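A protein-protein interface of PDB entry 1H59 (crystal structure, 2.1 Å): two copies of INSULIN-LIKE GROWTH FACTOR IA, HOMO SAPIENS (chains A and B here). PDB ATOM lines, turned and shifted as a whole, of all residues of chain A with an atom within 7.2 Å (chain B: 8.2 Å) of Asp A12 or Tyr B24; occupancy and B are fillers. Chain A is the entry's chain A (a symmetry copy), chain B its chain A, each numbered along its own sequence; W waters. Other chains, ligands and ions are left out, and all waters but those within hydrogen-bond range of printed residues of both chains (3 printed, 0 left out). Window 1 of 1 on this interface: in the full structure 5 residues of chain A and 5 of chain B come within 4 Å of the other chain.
Water W2 bridges the side-chain amide nitrogen (ND2) of Asn B26 (2.6 Å) and the side-chain carboxylate (OE2) of Glu A9 (3.1 Å). Water W3 bridges O of Phe B23 (2.7 Å) and OD1 of Asp A12 (2.9 Å). Water W1 bridges NE2 of Gln A15 (2.8 Å) and N of Phe B23 (3.1 Å).
The side-chain carboxylate (OD1) of Asp A12 sits at hydrogen-bond distance from the backbone NH (N) of Phe B25, at 2.8 Å. The side-chain carboxylate (OD2) of Asp A12 sits at hydrogen-bond distance from the backbone NH (N) of Asn B26 (2.8 Å).
Of the 14 printed residues of chain A, 5 touch a printed residue of chain B. Printed residues of chain A that touch a printed residue of chain B: Ala A8, Glu A9, Asp A12, Gln A15 and Phe A16. Hydrophobic or aromatic side chains of chain A that line the printed part of chain B: Ala A8 and Phe A16. Of the 24 printed residues of chain B, 5 touch a printed residue of chain A. Printed residues of chain B that touch a printed residue of chain A: Gly B22, Phe B23, Tyr B24, Phe B25 and Asn B26. Hydrophobic or aromatic side chains of chain B within 4 Å of the printed part of chain A: Tyr B24 and Phe B25. Among the printed residues, 10 pairs touch across the chains. Among the printed residues, no Asp or Glu carboxylate lies within 4 Å of a Lys or Arg side-chain nitrogen of the other chain.
The backbone carbonyl oxygen (O) of Asn B26 sits close to the backbone NH (N) of Gly B42 (3.4 Å). The backbone NH of Tyr B24 sits at hydrogen-bond distance from the backbone carbonyl oxygen of Tyr B60, at 2.8 Å. The backbone carbonyl oxygen (O) of Phe B25 lies within hydrogen-bond range of the backbone NH (N) of Ile B43 (3.0 Å). The backbone carbonyl oxygen of Gly B22 lies within hydrogen-bond range of the backbone NH of Ala B62 (2.8 Å). SG of Cys B61 forms a disulfide with SG of Cys B18 (2.0 Å).
Of chain B, only Tyr B24 (3.3 Å), Phe B25 (2.8 Å) and Asn B26 (2.8 Å) come within 4 Å of Asp A12. Of the printed residues of chain A, Tyr B24 touches Asp A12 (3.3 Å), Gln A15 (3.8 Å) and Phe A16 (3.6 Å). No residue of chain B comes within 4 Å of Ala A13. Of the printed residues of chain B, Gln A15 touches Gly B22, Phe B23 and Tyr B24. Printed residues of chain B within 4 Å of Phe A16: Tyr B24. Of the printed residues of chain A, Asn B26 touches Ala A8 (3.96 Å), Glu A9 (3.5 Å) and Asp A12 (2.8 Å). Ala B62 touches none of the printed residues of chain A. Pro B63 touches none of the printed residues of chain A. The nearest residue of chain B that does not touch Asp A12 is Lys B27 (4.1 Å). The nearest residue of chain A that does not touch Tyr B24 is Ala A13 (5.6 Å).
Among the printed residues, pairs that only touch across the chains: Ala A8 with Phe B25, Ala A8 with Asn B26, Glu A9 with Asn B26, Asp A12 with Tyr B24, Gln A15 with Gly B22, Gln A15 with Phe B23, Gln A15 with Tyr B24 and Phe A16 with Tyr B24.
Positions printed for both chains: 14, 18 and 23. Of the 10 pairs that touch across the chains among the printed residues, none has its exchanged pair printed and touching as well.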
ATOM      1  N   LEU A   5     -20.066 -13.274 -21.116  1.00  0.00           N
ATOM      2  CA  LEU A   5     -19.562 -11.914 -21.228  1.00  0.00           C
ATOM      3  C   LEU A   5     -20.701 -10.959 -20.900  1.00  0.00           C
ATOM      4  O   LEU A   5     -21.790 -11.072 -21.461  1.00  0.00           O
ATOM      5  CB  LEU A   5     -19.068 -11.626 -22.650  1.00  0.00           C
ATOM      6  CG  LEU A   5     -17.570 -11.585 -22.947  1.00  0.00           C
ATOM      7  CD1 LEU A   5     -17.368 -10.938 -24.321  1.00  0.00           C
ATOM      8  CD2 LEU A   5     -16.836 -10.790 -21.874  1.00  0.00           C
ATOM      9  N   GLY A   7     -21.807  -6.683 -19.390  1.00  0.00           N
ATOM     10  CA  GLY A   7     -21.434  -5.282 -19.305  1.00  0.00           C
ATOM     11  C   GLY A   7     -20.611  -4.644 -20.407  1.00  0.00           C
ATOM     12  O   GLY A   7     -20.797  -4.901 -21.602  1.00  0.00           O
ATOM     13  N   ALA A   8     -19.705  -3.772 -19.983  1.00  0.00           N
ATOM     14  CA  ALA A   8     -18.839  -3.038 -20.895  1.00  0.00           C
ATOM     15  C   ALA A   8     -18.020  -3.981 -21.761  1.00  0.00           C
ATOM     16  O   ALA A   8     -17.786  -3.707 -22.931  1.00  0.00           O
ATOM     17  CB  ALA A   8     -17.921  -2.106 -20.103  1.00  0.00           C
ATOM     18  N   GLU A   9     -17.589  -5.104 -21.197  1.00  0.00           N
ATOM     19  CA  GLU A   9     -16.799  -6.047 -21.980  1.00  0.00           C
ATOM     20  C   GLU A   9     -17.593  -6.666 -23.116  1.00  0.00           C
ATOM     21  O   GLU A   9     -17.045  -6.934 -24.179  1.00  0.00           O
ATOM     22  CB  GLU A   9     -16.231  -7.149 -21.092  1.00  0.00           C
ATOM     23  CG  GLU A   9     -15.153  -6.663 -20.151  1.00  0.00           C
ATOM     24  CD  GLU A   9     -14.501  -7.800 -19.408  1.00  0.00           C
ATOM     25  OE1 GLU A   9     -15.229  -8.545 -18.719  1.00  0.00           O
ATOM     26  OE2 GLU A   9     -13.265  -7.950 -19.517  1.00  0.00           O
ATOM     27  N   LEU A  10     -18.880  -6.910 -22.892  1.00  0.00           N
ATOM     28  CA  LEU A  10     -19.722  -7.488 -23.929  1.00  0.00           C
ATOM     29  C   LEU A  10     -19.883  -6.482 -25.082  1.00  0.00           C
ATOM     30  O   LEU A  10     -19.855  -6.845 -26.260  1.00  0.00           O
ATOM     31  CB  LEU A  10     -21.096  -7.855 -23.355  1.00  0.00           C
ATOM     32  CG  LEU A  10     -22.119  -8.284 -24.411  1.00  0.00           C
ATOM     33  CD1 LEU A  10     -21.589  -9.497 -25.162  1.00  0.00           C
ATOM     34  CD2 LEU A  10     -23.461  -8.594 -23.752  1.00  0.00           C
ATOM     35  N   VAL A  11     -20.070  -5.218 -24.729  1.00  0.00           N
ATOM     36  CA  VAL A  11     -20.220  -4.166 -25.726  1.00  0.00           C
ATOM     37  C   VAL A  11     -18.916  -3.986 -26.503  1.00  0.00           C
ATOM     38  O   VAL A  11     -18.932  -3.843 -27.720  1.00  0.00           O
ATOM     39  CB  VAL A  11     -20.627  -2.825 -25.068  1.00  0.00           C
ATOM     40  CG1 VAL A  11     -20.646  -1.707 -26.106  1.00  0.00           C
ATOM     41  CG2 VAL A  11     -22.013  -2.964 -24.442  1.00  0.00           C
ATOM     42  N   ASP A  12     -17.784  -4.001 -25.807  1.00  0.00           N
ATOM     43  CA  ASP A  12     -16.507  -3.849 -26.496  1.00  0.00           C
ATOM     44  C   ASP A  12     -16.272  -5.003 -27.468  1.00  0.00           C
ATOM     45  O   ASP A  12     -15.794  -4.787 -28.578  1.00  0.00           O
ATOM     46  CB  ASP A  12     -15.353  -3.767 -25.491  1.00  0.00           C
ATOM     47  CG  ASP A  12     -15.339  -2.451 -24.731  1.00  0.00           C
ATOM     48  OD1 ASP A  12     -16.054  -1.514 -25.143  1.00  0.00           O
ATOM     49  OD2 ASP A  12     -14.608  -2.349 -23.728  1.00  0.00           O
ATOM     50  N   ALA A  13     -16.611  -6.221 -27.048  1.00  0.00           N
ATOM     51  CA  ALA A  13     -16.446  -7.399 -27.903  1.00  0.00           C
ATOM     52  C   ALA A  13     -17.299  -7.272 -29.168  1.00  0.00           C
ATOM     53  O   ALA A  13     -16.857  -7.628 -30.259  1.00  0.00           O
ATOM     54  CB  ALA A  13     -16.824  -8.682 -27.125  1.00  0.00           C
ATOM     55  N   LEU A  14     -18.524  -6.771 -29.017  1.00  0.00           N
ATOM     56  CA  LEU A  14     -19.427  -6.576 -30.154  1.00  0.00           C
ATOM     57  C   LEU A  14     -18.865  -5.548 -31.135  1.00  0.00           C
ATOM     58  O   LEU A  14     -18.909  -5.736 -32.355  1.00  0.00           O
ATOM     59  CB  LEU A  14     -20.805  -6.113 -29.669  1.00  0.00           C
ATOM     60  CG  LEU A  14     -21.729  -7.220 -29.165  1.00  0.00           C
ATOM     61  CD1 LEU A  14     -22.868  -6.631 -28.358  1.00  0.00           C
ATOM     62  CD2 LEU A  14     -22.245  -8.013 -30.353  1.00  0.00           C
ATOM     63  N   GLN A  15     -18.351  -4.452 -30.592  1.00  0.00           N
ATOM     64  CA  GLN A  15     -17.762  -3.396 -31.404  1.00  0.00           C
ATOM     65  C   GLN A  15     -16.561  -3.954 -32.169  1.00  0.00           C
ATOM     66  O   GLN A  15     -16.357  -3.639 -33.342  1.00  0.00           O
ATOM     67  CB  GLN A  15     -17.309  -2.235 -30.509  1.00  0.00           C
ATOM     68  CG  GLN A  15     -16.519  -1.173 -31.252  1.00  0.00           C
ATOM     69  CD  GLN A  15     -17.377  -0.370 -32.216  1.00  0.00           C
ATOM     70  OE1 GLN A  15     -16.917   0.034 -33.283  1.00  0.00           O
ATOM     71  NE2 GLN A  15     -18.623  -0.125 -31.837  1.00  0.00           N
ATOM     72  N   PHE A  16     -15.776  -4.796 -31.504  1.00  0.00           N
ATOM     73  CA  PHE A  16     -14.600  -5.387 -32.138  1.00  0.00           C
ATOM     74  C   PHE A  16     -14.998  -6.361 -33.253  1.00  0.00           C
ATOM     75  O   PHE A  16     -14.482  -6.290 -34.365  1.00  0.00           O
ATOM     76  CB  PHE A  16     -13.740  -6.118 -31.097  1.00  0.00           C
ATOM     77  CG  PHE A  16     -12.462  -6.688 -31.662  1.00  0.00           C
ATOM     78  CD1 PHE A  16     -11.490  -5.848 -32.199  1.00  0.00           C
ATOM     79  CD2 PHE A  16     -12.240  -8.061 -31.673  1.00  0.00           C
ATOM     80  CE1 PHE A  16     -10.311  -6.367 -32.741  1.00  0.00           C
ATOM     81  CE2 PHE A  16     -11.063  -8.593 -32.213  1.00  0.00           C
ATOM     82  CZ  PHE A  16     -10.098  -7.744 -32.747  1.00  0.00           C
ATOM     83  N   VAL A  17     -15.930  -7.260 -32.957  1.00  0.00           N
ATOM     84  CA  VAL A  17     -16.370  -8.245 -33.940  1.00  0.00           C
ATOM     85  C   VAL A  17     -17.118  -7.636 -35.126  1.00  0.00           C
ATOM     86  O   VAL A  17     -16.832  -7.956 -36.275  1.00  0.00           O
ATOM     87  CB  VAL A  17     -17.263  -9.322 -33.272  1.00  0.00           C
ATOM     88  CG1 VAL A  17     -17.861 -10.252 -34.319  1.00  0.00           C
ATOM     89  CG2 VAL A  17     -16.443 -10.117 -32.279  1.00  0.00           C
ATOM     90  N   CYS A  18     -18.061  -6.744 -34.843  1.00  0.00           N
ATOM     91  CA  CYS A  18     -18.876  -6.119 -35.884  1.00  0.00           C
ATOM     92  C   CYS A  18     -18.265  -4.921 -36.613  1.00  0.00           C
ATOM     93  O   CYS A  18     -18.614  -4.653 -37.759  1.00  0.00           O
ATOM     94  CB  CYS A  18     -20.226  -5.720 -35.292  1.00  0.00           C
ATOM     95  SG  CYS A  18     -21.110  -7.109 -34.523  1.00  0.00           S
ATOM     96  N   PHE A  23     -24.229  -2.973 -34.651  1.00  0.00           N
ATOM     97  CA  PHE A  23     -24.864  -4.182 -34.139  1.00  0.00           C
ATOM     98  C   PHE A  23     -26.162  -3.903 -33.391  1.00  0.00           C
ATOM     99  O   PHE A  23     -26.480  -2.753 -33.078  1.00  0.00           O
ATOM    100  CB  PHE A  23     -23.875  -4.921 -33.224  1.00  0.00           C
ATOM    101  CG  PHE A  23     -23.278  -4.051 -32.143  1.00  0.00           C
ATOM    102  CD1 PHE A  23     -23.930  -3.880 -30.927  1.00  0.00           C
ATOM    103  CD2 PHE A  23     -22.075  -3.377 -32.358  1.00  0.00           C
ATOM    104  CE1 PHE A  23     -23.399  -3.053 -29.933  1.00  0.00           C
ATOM    105  CE2 PHE A  23     -21.531  -2.544 -31.371  1.00  0.00           C
ATOM    106  CZ  PHE A  23     -22.193  -2.382 -30.158  1.00  0.00           C
ATOM    107  N   LEU B  14     -18.100  10.956 -26.538  1.00  0.00           N
ATOM    108  CA  LEU B  14     -17.281   9.918 -27.168  1.00  0.00           C
ATOM    109  C   LEU B  14     -17.617   9.772 -28.651  1.00  0.00           C
ATOM    110  O   LEU B  14     -16.729   9.650 -29.500  1.00  0.00           O
ATOM    111  CB  LEU B  14     -17.492   8.573 -26.466  1.00  0.00           C
ATOM    112  CG  LEU B  14     -16.698   8.374 -25.175  1.00  0.00           C
ATOM    113  CD1 LEU B  14     -17.270   7.220 -24.376  1.00  0.00           C
ATOM    114  CD2 LEU B  14     -15.239   8.135 -25.523  1.00  0.00           C
ATOM    115  N   CYS B  18     -14.745  10.508 -31.303  1.00  0.00           N
ATOM    116  CA  CYS B  18     -14.328   9.355 -32.099  1.00  0.00           C
ATOM    117  C   CYS B  18     -14.958   9.207 -33.485  1.00  0.00           C
ATOM    118  O   CYS B  18     -14.356   8.611 -34.374  1.00  0.00           O
ATOM    119  CB  CYS B  18     -14.566   8.078 -31.292  1.00  0.00           C
ATOM    120  SG  CYS B  18     -13.736   8.088 -29.676  1.00  0.00           S
ATOM    121  N   ARG B  21     -14.969   6.039 -36.210  1.00  0.00           N
ATOM    122  CA  ARG B  21     -14.004   5.056 -35.723  1.00  0.00           C
ATOM    123  C   ARG B  21     -14.647   4.128 -34.695  1.00  0.00           C
ATOM    124  O   ARG B  21     -14.322   2.947 -34.622  1.00  0.00           O
ATOM    125  CB  ARG B  21     -12.816   5.752 -35.067  1.00  0.00           C
ATOM    126  CG  ARG B  21     -12.020   6.642 -35.994  1.00  0.00           C
ATOM    127  CD  ARG B  21     -11.029   7.461 -35.199  1.00  0.00           C
ATOM    128  NE  ARG B  21     -10.147   6.612 -34.409  1.00  0.00           N
ATOM    129  CZ  ARG B  21      -9.245   7.073 -33.551  1.00  0.00           C
ATOM    130  NH1 ARG B  21      -9.108   8.379 -33.373  1.00  0.00           N
ATOM    131  NH2 ARG B  21      -8.476   6.228 -32.874  1.00  0.00           N
ATOM    132  N   GLY B  22     -15.569   4.661 -33.904  1.00  0.00           N
ATOM    133  CA  GLY B  22     -16.190   3.845 -32.879  1.00  0.00           C
ATOM    134  C   GLY B  22     -15.320   3.966 -31.644  1.00  0.00           C
ATOM    135  O   GLY B  22     -14.256   4.574 -31.706  1.00  0.00           O
ATOM    136  N   PHE B  23     -15.749   3.389 -30.527  1.00  0.00           N
ATOM    137  CA  PHE B  23     -14.973   3.490 -29.296  1.00  0.00           C
ATOM    138  C   PHE B  23     -15.232   2.339 -28.331  1.00  0.00           C
ATOM    139  O   PHE B  23     -16.170   1.559 -28.511  1.00  0.00           O
ATOM    140  CB  PHE B  23     -15.284   4.832 -28.615  1.00  0.00           C
ATOM    141  CG  PHE B  23     -16.760   5.088 -28.419  1.00  0.00           C
ATOM    142  CD1 PHE B  23     -17.419   4.616 -27.289  1.00  0.00           C
ATOM    143  CD2 PHE B  23     -17.494   5.778 -29.383  1.00  0.00           C
ATOM    144  CE1 PHE B  23     -18.791   4.824 -27.116  1.00  0.00           C
ATOM    145  CE2 PHE B  23     -18.870   5.992 -29.223  1.00  0.00           C
ATOM    146  CZ  PHE B  23     -19.518   5.515 -28.089  1.00  0.00           C
ATOM    147  N   TYR B  24     -14.390   2.240 -27.309  1.00  0.00           N
ATOM    148  CA  TYR B  24     -14.518   1.194 -26.300  1.00  0.00           C
ATOM    149  C   TYR B  24     -14.829   1.792 -24.943  1.00  0.00           C
ATOM    150  O   TYR B  24     -14.611   2.985 -24.713  1.00  0.00           O
ATOM    151  CB  TYR B  24     -13.229   0.382 -26.192  1.00  0.00           C
ATOM    152  CG  TYR B  24     -12.891  -0.389 -27.437  1.00  0.00           C
ATOM    153  CD1 TYR B  24     -13.784  -1.321 -27.968  1.00  0.00           C
ATOM    154  CD2 TYR B  24     -11.681  -0.186 -28.093  1.00  0.00           C
ATOM    155  CE1 TYR B  24     -13.479  -2.027 -29.121  1.00  0.00           C
ATOM    156  CE2 TYR B  24     -11.366  -0.891 -29.246  1.00  0.00           C
ATOM    157  CZ  TYR B  24     -12.266  -1.804 -29.754  1.00  0.00           C
ATOM    158  OH  TYR B  24     -11.948  -2.488 -30.901  1.00  0.00           O
ATOM    159  N   PHE B  25     -15.324   0.947 -24.042  1.00  0.00           N
ATOM    160  CA  PHE B  25     -15.666   1.370 -22.692  1.00  0.00           C
ATOM    161  C   PHE B  25     -14.769   0.823 -21.588  1.00  0.00           C
ATOM    162  O   PHE B  25     -14.345   1.563 -20.698  1.00  0.00           O
ATOM    163  CB  PHE B  25     -17.101   0.958 -22.340  1.00  0.00           C
ATOM    164  CG  PHE B  25     -18.153   1.767 -23.017  1.00  0.00           C
ATOM    165  CD1 PHE B  25     -18.814   1.275 -24.138  1.00  0.00           C
ATOM    166  CD2 PHE B  25     -18.501   3.022 -22.528  1.00  0.00           C
ATOM    167  CE1 PHE B  25     -19.810   2.023 -24.762  1.00  0.00           C
ATOM    168  CE2 PHE B  25     -19.497   3.779 -23.148  1.00  0.00           C
ATOM    169  CZ  PHE B  25     -20.152   3.276 -24.266  1.00  0.00           C
ATOM    170  N   ASN B  26     -14.484  -0.474 -21.636  1.00  0.00           N
ATOM    171  CA  ASN B  26     -13.716  -1.102 -20.564  1.00  0.00           C
ATOM    172  C   ASN B  26     -12.225  -0.829 -20.489  1.00  0.00           C
ATOM    173  O   ASN B  26     -11.656  -0.806 -19.398  1.00  0.00           O
ATOM    174  CB  ASN B  26     -13.959  -2.612 -20.563  1.00  0.00           C
ATOM    175  CG  ASN B  26     -13.828  -3.210 -19.176  1.00  0.00           C
ATOM    176  OD1 ASN B  26     -14.488  -2.762 -18.240  1.00  0.00           O
ATOM    177  ND2 ASN B  26     -12.981  -4.215 -19.034  1.00  0.00           N
ATOM    178  N   LYS B  27     -11.588  -0.633 -21.637  1.00  0.00           N
ATOM    179  CA  LYS B  27     -10.157  -0.368 -21.661  1.00  0.00           C
ATOM    180  C   LYS B  27      -9.852   0.592 -22.793  1.00  0.00           C
ATOM    181  O   LYS B  27     -10.583   0.644 -23.781  1.00  0.00           O
ATOM    182  CB  LYS B  27      -9.368  -1.661 -21.897  1.00  0.00           C
ATOM    183  CG  LYS B  27      -9.622  -2.771 -20.899  1.00  0.00           C
ATOM    184  CD  LYS B  27      -9.036  -2.440 -19.537  1.00  0.00           C
ATOM    185  CE  LYS B  27      -9.136  -3.637 -18.602  1.00  0.00           C
ATOM    186  NZ  LYS B  27      -8.549  -3.338 -17.263  1.00  0.00           N
ATOM    187  N   PRO B  28      -8.775   1.380 -22.659  1.00  0.00           N
ATOM    188  CA  PRO B  28      -8.401   2.326 -23.710  1.00  0.00           C
ATOM    189  C   PRO B  28      -7.687   1.530 -24.796  1.00  0.00           C
ATOM    190  O   PRO B  28      -7.166   0.442 -24.530  1.00  0.00           O
ATOM    191  CB  PRO B  28      -7.462   3.285 -22.989  1.00  0.00           C
ATOM    192  CG  PRO B  28      -6.767   2.382 -22.017  1.00  0.00           C
ATOM    193  CD  PRO B  28      -7.908   1.540 -21.476  1.00  0.00           C
ATOM    194  N   THR B  29      -7.672   2.056 -26.014  1.00  0.00           N
ATOM    195  CA  THR B  29      -7.005   1.372 -27.114  1.00  0.00           C
ATOM    196  C   THR B  29      -5.498   1.508 -26.935  1.00  0.00           C
ATOM    197  O   THR B  29      -5.015   2.531 -26.451  1.00  0.00           O
ATOM    198  CB  THR B  29      -7.409   1.975 -28.478  1.00  0.00           C
ATOM    199  OG1 THR B  29      -8.800   1.724 -28.719  1.00  0.00           O
ATOM    200  CG2 THR B  29      -6.587   1.357 -29.604  1.00  0.00           C
ATOM    201  N   GLY B  30      -4.763   0.465 -27.304  1.00  0.00           N
ATOM    202  CA  GLY B  30      -3.317   0.507 -27.189  1.00  0.00           C
ATOM    203  C   GLY B  30      -2.777   0.210 -25.805  1.00  0.00           C
ATOM    204  O   GLY B  30      -2.953  -0.893 -25.288  1.00  0.00           O
ATOM    205  N   THR B  41      -7.845   1.566 -17.030  1.00  0.00           N
ATOM    206  CA  THR B  41      -9.203   1.289 -16.477  1.00  0.00           C
ATOM    207  C   THR B  41     -10.275   1.711 -17.485  1.00  0.00           C
ATOM    208  O   THR B  41      -9.953   2.075 -18.615  1.00  0.00           O
ATOM    209  CB  THR B  41      -9.416   2.048 -15.158  1.00  0.00           C
ATOM    210  OG1 THR B  41     -10.527   1.483 -14.447  1.00  0.00           O
ATOM    211  CG2 THR B  41      -9.699   3.514 -15.440  1.00  0.00           C
ATOM    212  N   GLY B  42     -11.541   1.663 -17.070  1.00  0.00           N
ATOM    213  CA  GLY B  42     -12.640   2.021 -17.956  1.00  0.00           C
ATOM    214  C   GLY B  42     -12.940   3.508 -18.028  1.00  0.00           C
ATOM    215  O   GLY B  42     -12.655   4.254 -17.093  1.00  0.00           O
ATOM    216  N   ILE B  43     -13.537   3.938 -19.138  1.00  0.00           N
ATOM    217  CA  ILE B  43     -13.861   5.351 -19.334  1.00  0.00           C
ATOM    218  C   ILE B  43     -14.877   5.911 -18.319  1.00  0.00           C
ATOM    219  O   ILE B  43     -14.774   7.069 -17.915  1.00  0.00           O
ATOM    220  CB  ILE B  43     -14.374   5.608 -20.781  1.00  0.00           C
ATOM    221  CG1 ILE B  43     -14.504   7.115 -21.034  1.00  0.00           C
ATOM    222  CG2 ILE B  43     -15.715   4.914 -21.004  1.00  0.00           C
ATOM    223  CD1 ILE B  43     -13.185   7.851 -21.058  1.00  0.00           C
ATOM    224  N   VAL B  44     -15.855   5.106 -17.913  1.00  0.00           N
ATOM    225  CA  VAL B  44     -16.844   5.563 -16.928  1.00  0.00           C
ATOM    226  C   VAL B  44     -16.152   5.858 -15.599  1.00  0.00           C
ATOM    227  O   VAL B  44     -16.419   6.882 -14.965  1.00  0.00           O
ATOM    228  CB  VAL B  44     -17.944   4.508 -16.674  1.00  0.00           C
ATOM    229  CG1 VAL B  44     -18.832   4.952 -15.514  1.00  0.00           C
ATOM    230  CG2 VAL B  44     -18.782   4.314 -17.929  1.00  0.00           C
ATOM    231  N   ARG B  56      -8.290  12.243 -22.719  1.00  0.00           N
ATOM    232  CA  ARG B  56      -8.736  10.989 -22.128  1.00  0.00           C
ATOM    233  C   ARG B  56      -9.733  10.284 -23.056  1.00  0.00           C
ATOM    234  O   ARG B  56      -9.643   9.075 -23.276  1.00  0.00           O
ATOM    235  CB  ARG B  56      -9.395  11.257 -20.774  1.00  0.00           C
ATOM    236  CG  ARG B  56      -9.801   9.997 -20.026  1.00  0.00           C
ATOM    237  CD  ARG B  56      -8.581   9.258 -19.506  1.00  0.00           C
ATOM    238  NE  ARG B  56      -7.890  10.018 -18.468  1.00  0.00           N
ATOM    239  CZ  ARG B  56      -6.748   9.642 -17.902  1.00  0.00           C
ATOM    240  NH1 ARG B  56      -6.162   8.511 -18.275  1.00  0.00           N
ATOM    241  NH2 ARG B  56      -6.195  10.393 -16.959  1.00  0.00           N
ATOM    242  N   LEU B  57     -10.673  11.054 -23.603  1.00  0.00           N
ATOM    243  CA  LEU B  57     -11.694  10.523 -24.504  1.00  0.00           C
ATOM    244  C   LEU B  57     -11.106   9.871 -25.753  1.00  0.00           C
ATOM    245  O   LEU B  57     -11.504   8.770 -26.134  1.00  0.00           O
ATOM    246  CB  LEU B  57     -12.667  11.644 -24.919  1.00  0.00           C
ATOM    247  CG  LEU B  57     -13.595  12.159 -23.807  1.00  0.00           C
ATOM    248  CD1 LEU B  57     -14.341  13.405 -24.265  1.00  0.00           C
ATOM    249  CD2 LEU B  57     -14.583  11.069 -23.424  1.00  0.00           C
ATOM    250  N   GLU B  58     -10.153  10.549 -26.384  1.00  0.00           N
ATOM    251  CA  GLU B  58      -9.531  10.034 -27.600  1.00  0.00           C
ATOM    252  C   GLU B  58      -8.806   8.708 -27.392  1.00  0.00           C
ATOM    253  O   GLU B  58      -8.681   7.915 -28.321  1.00  0.00           O
ATOM    254  CB  GLU B  58      -8.565  11.074 -28.178  1.00  0.00           C
ATOM    255  CG  GLU B  58      -9.258  12.353 -28.604  1.00  0.00           C
ATOM    256  CD  GLU B  58      -8.321  13.333 -29.279  1.00  0.00           C
ATOM    257  OE1 GLU B  58      -7.747  12.975 -30.329  1.00  0.00           O
ATOM    258  OE2 GLU B  58      -8.161  14.458 -28.758  1.00  0.00           O
ATOM    259  N   MET B  59      -8.338   8.460 -26.177  1.00  0.00           N
ATOM    260  CA  MET B  59      -7.642   7.213 -25.884  1.00  0.00           C
ATOM    261  C   MET B  59      -8.566   6.003 -26.042  1.00  0.00           C
ATOM    262  O   MET B  59      -8.101   4.890 -26.290  1.00  0.00           O
ATOM    263  CB  MET B  59      -7.098   7.232 -24.454  1.00  0.00           C
ATOM    264  CG  MET B  59      -5.978   8.221 -24.205  1.00  0.00           C
ATOM    265  SD  MET B  59      -5.540   8.222 -22.451  1.00  0.00           S
ATOM    266  CE  MET B  59      -4.850   6.562 -22.264  1.00  0.00           C
ATOM    267  N   TYR B  60      -9.870   6.220 -25.897  1.00  0.00           N
ATOM    268  CA  TYR B  60     -10.828   5.125 -26.002  1.00  0.00           C
ATOM    269  C   TYR B  60     -11.429   4.924 -27.384  1.00  0.00           C
ATOM    270  O   TYR B  60     -12.223   4.007 -27.583  1.00  0.00           O
ATOM    271  CB  TYR B  60     -11.944   5.287 -24.957  1.00  0.00           C
ATOM    272  CG  TYR B  60     -11.447   5.086 -23.537  1.00  0.00           C
ATOM    273  CD1 TYR B  60     -10.754   6.099 -22.870  1.00  0.00           C
ATOM    274  CD2 TYR B  60     -11.625   3.865 -22.878  1.00  0.00           C
ATOM    275  CE1 TYR B  60     -10.251   5.902 -21.589  1.00  0.00           C
ATOM    276  CE2 TYR B  60     -11.119   3.656 -21.595  1.00  0.00           C
ATOM    277  CZ  TYR B  60     -10.434   4.681 -20.957  1.00  0.00           C
ATOM    278  OH  TYR B  60      -9.925   4.484 -19.696  1.00  0.00           O
ATOM    279  N   CYS B  61     -11.057   5.772 -28.342  1.00  0.00           N
ATOM    280  CA  CYS B  61     -11.563   5.615 -29.702  1.00  0.00           C
ATOM    281  C   CYS B  61     -10.952   4.332 -30.260  1.00  0.00           C
ATOM    282  O   CYS B  61      -9.857   3.945 -29.867  1.00  0.00           O
ATOM    283  CB  CYS B  61     -11.142   6.793 -30.594  1.00  0.00           C
ATOM    284  SG  CYS B  61     -11.790   8.442 -30.144  1.00  0.00           S
ATOM    285  N   ALA B  62     -11.658   3.670 -31.169  1.00  0.00           N
ATOM    286  CA  ALA B  62     -11.141   2.445 -31.769  1.00  0.00           C
ATOM    287  C   ALA B  62     -10.099   2.803 -32.838  1.00  0.00           C
ATOM    288  O   ALA B  62     -10.035   3.945 -33.298  1.00  0.00           O
ATOM    289  CB  ALA B  62     -12.282   1.638 -32.386  1.00  0.00           C
ATOM    290  N   PRO B  63      -9.258   1.831 -33.235  1.00  0.00           N
ATOM    291  CA  PRO B  63      -8.213   2.041 -34.247  1.00  0.00           C
ATOM    292  C   PRO B  63      -8.695   2.199 -35.690  1.00  0.00           C
ATOM    293  O   PRO B  63      -9.830   1.860 -36.024  1.00  0.00           O
ATOM    294  CB  PRO B  63      -7.327   0.801 -34.100  1.00  0.00           C
ATOM    295  CG  PRO B  63      -7.574   0.350 -32.694  1.00  0.00           C
ATOM    296  CD  PRO B  63      -9.060   0.538 -32.559  1.00  0.00           C
HETATM  297  O   HOH W   1     -18.694   2.438 -30.595  1.00  0.00           O
HETATM  298  O   HOH W   2     -12.135  -5.590 -21.093  1.00  0.00           O
HETATM  299  O   HOH W   3     -17.607  -0.427 -27.303  1.00  0.00           O
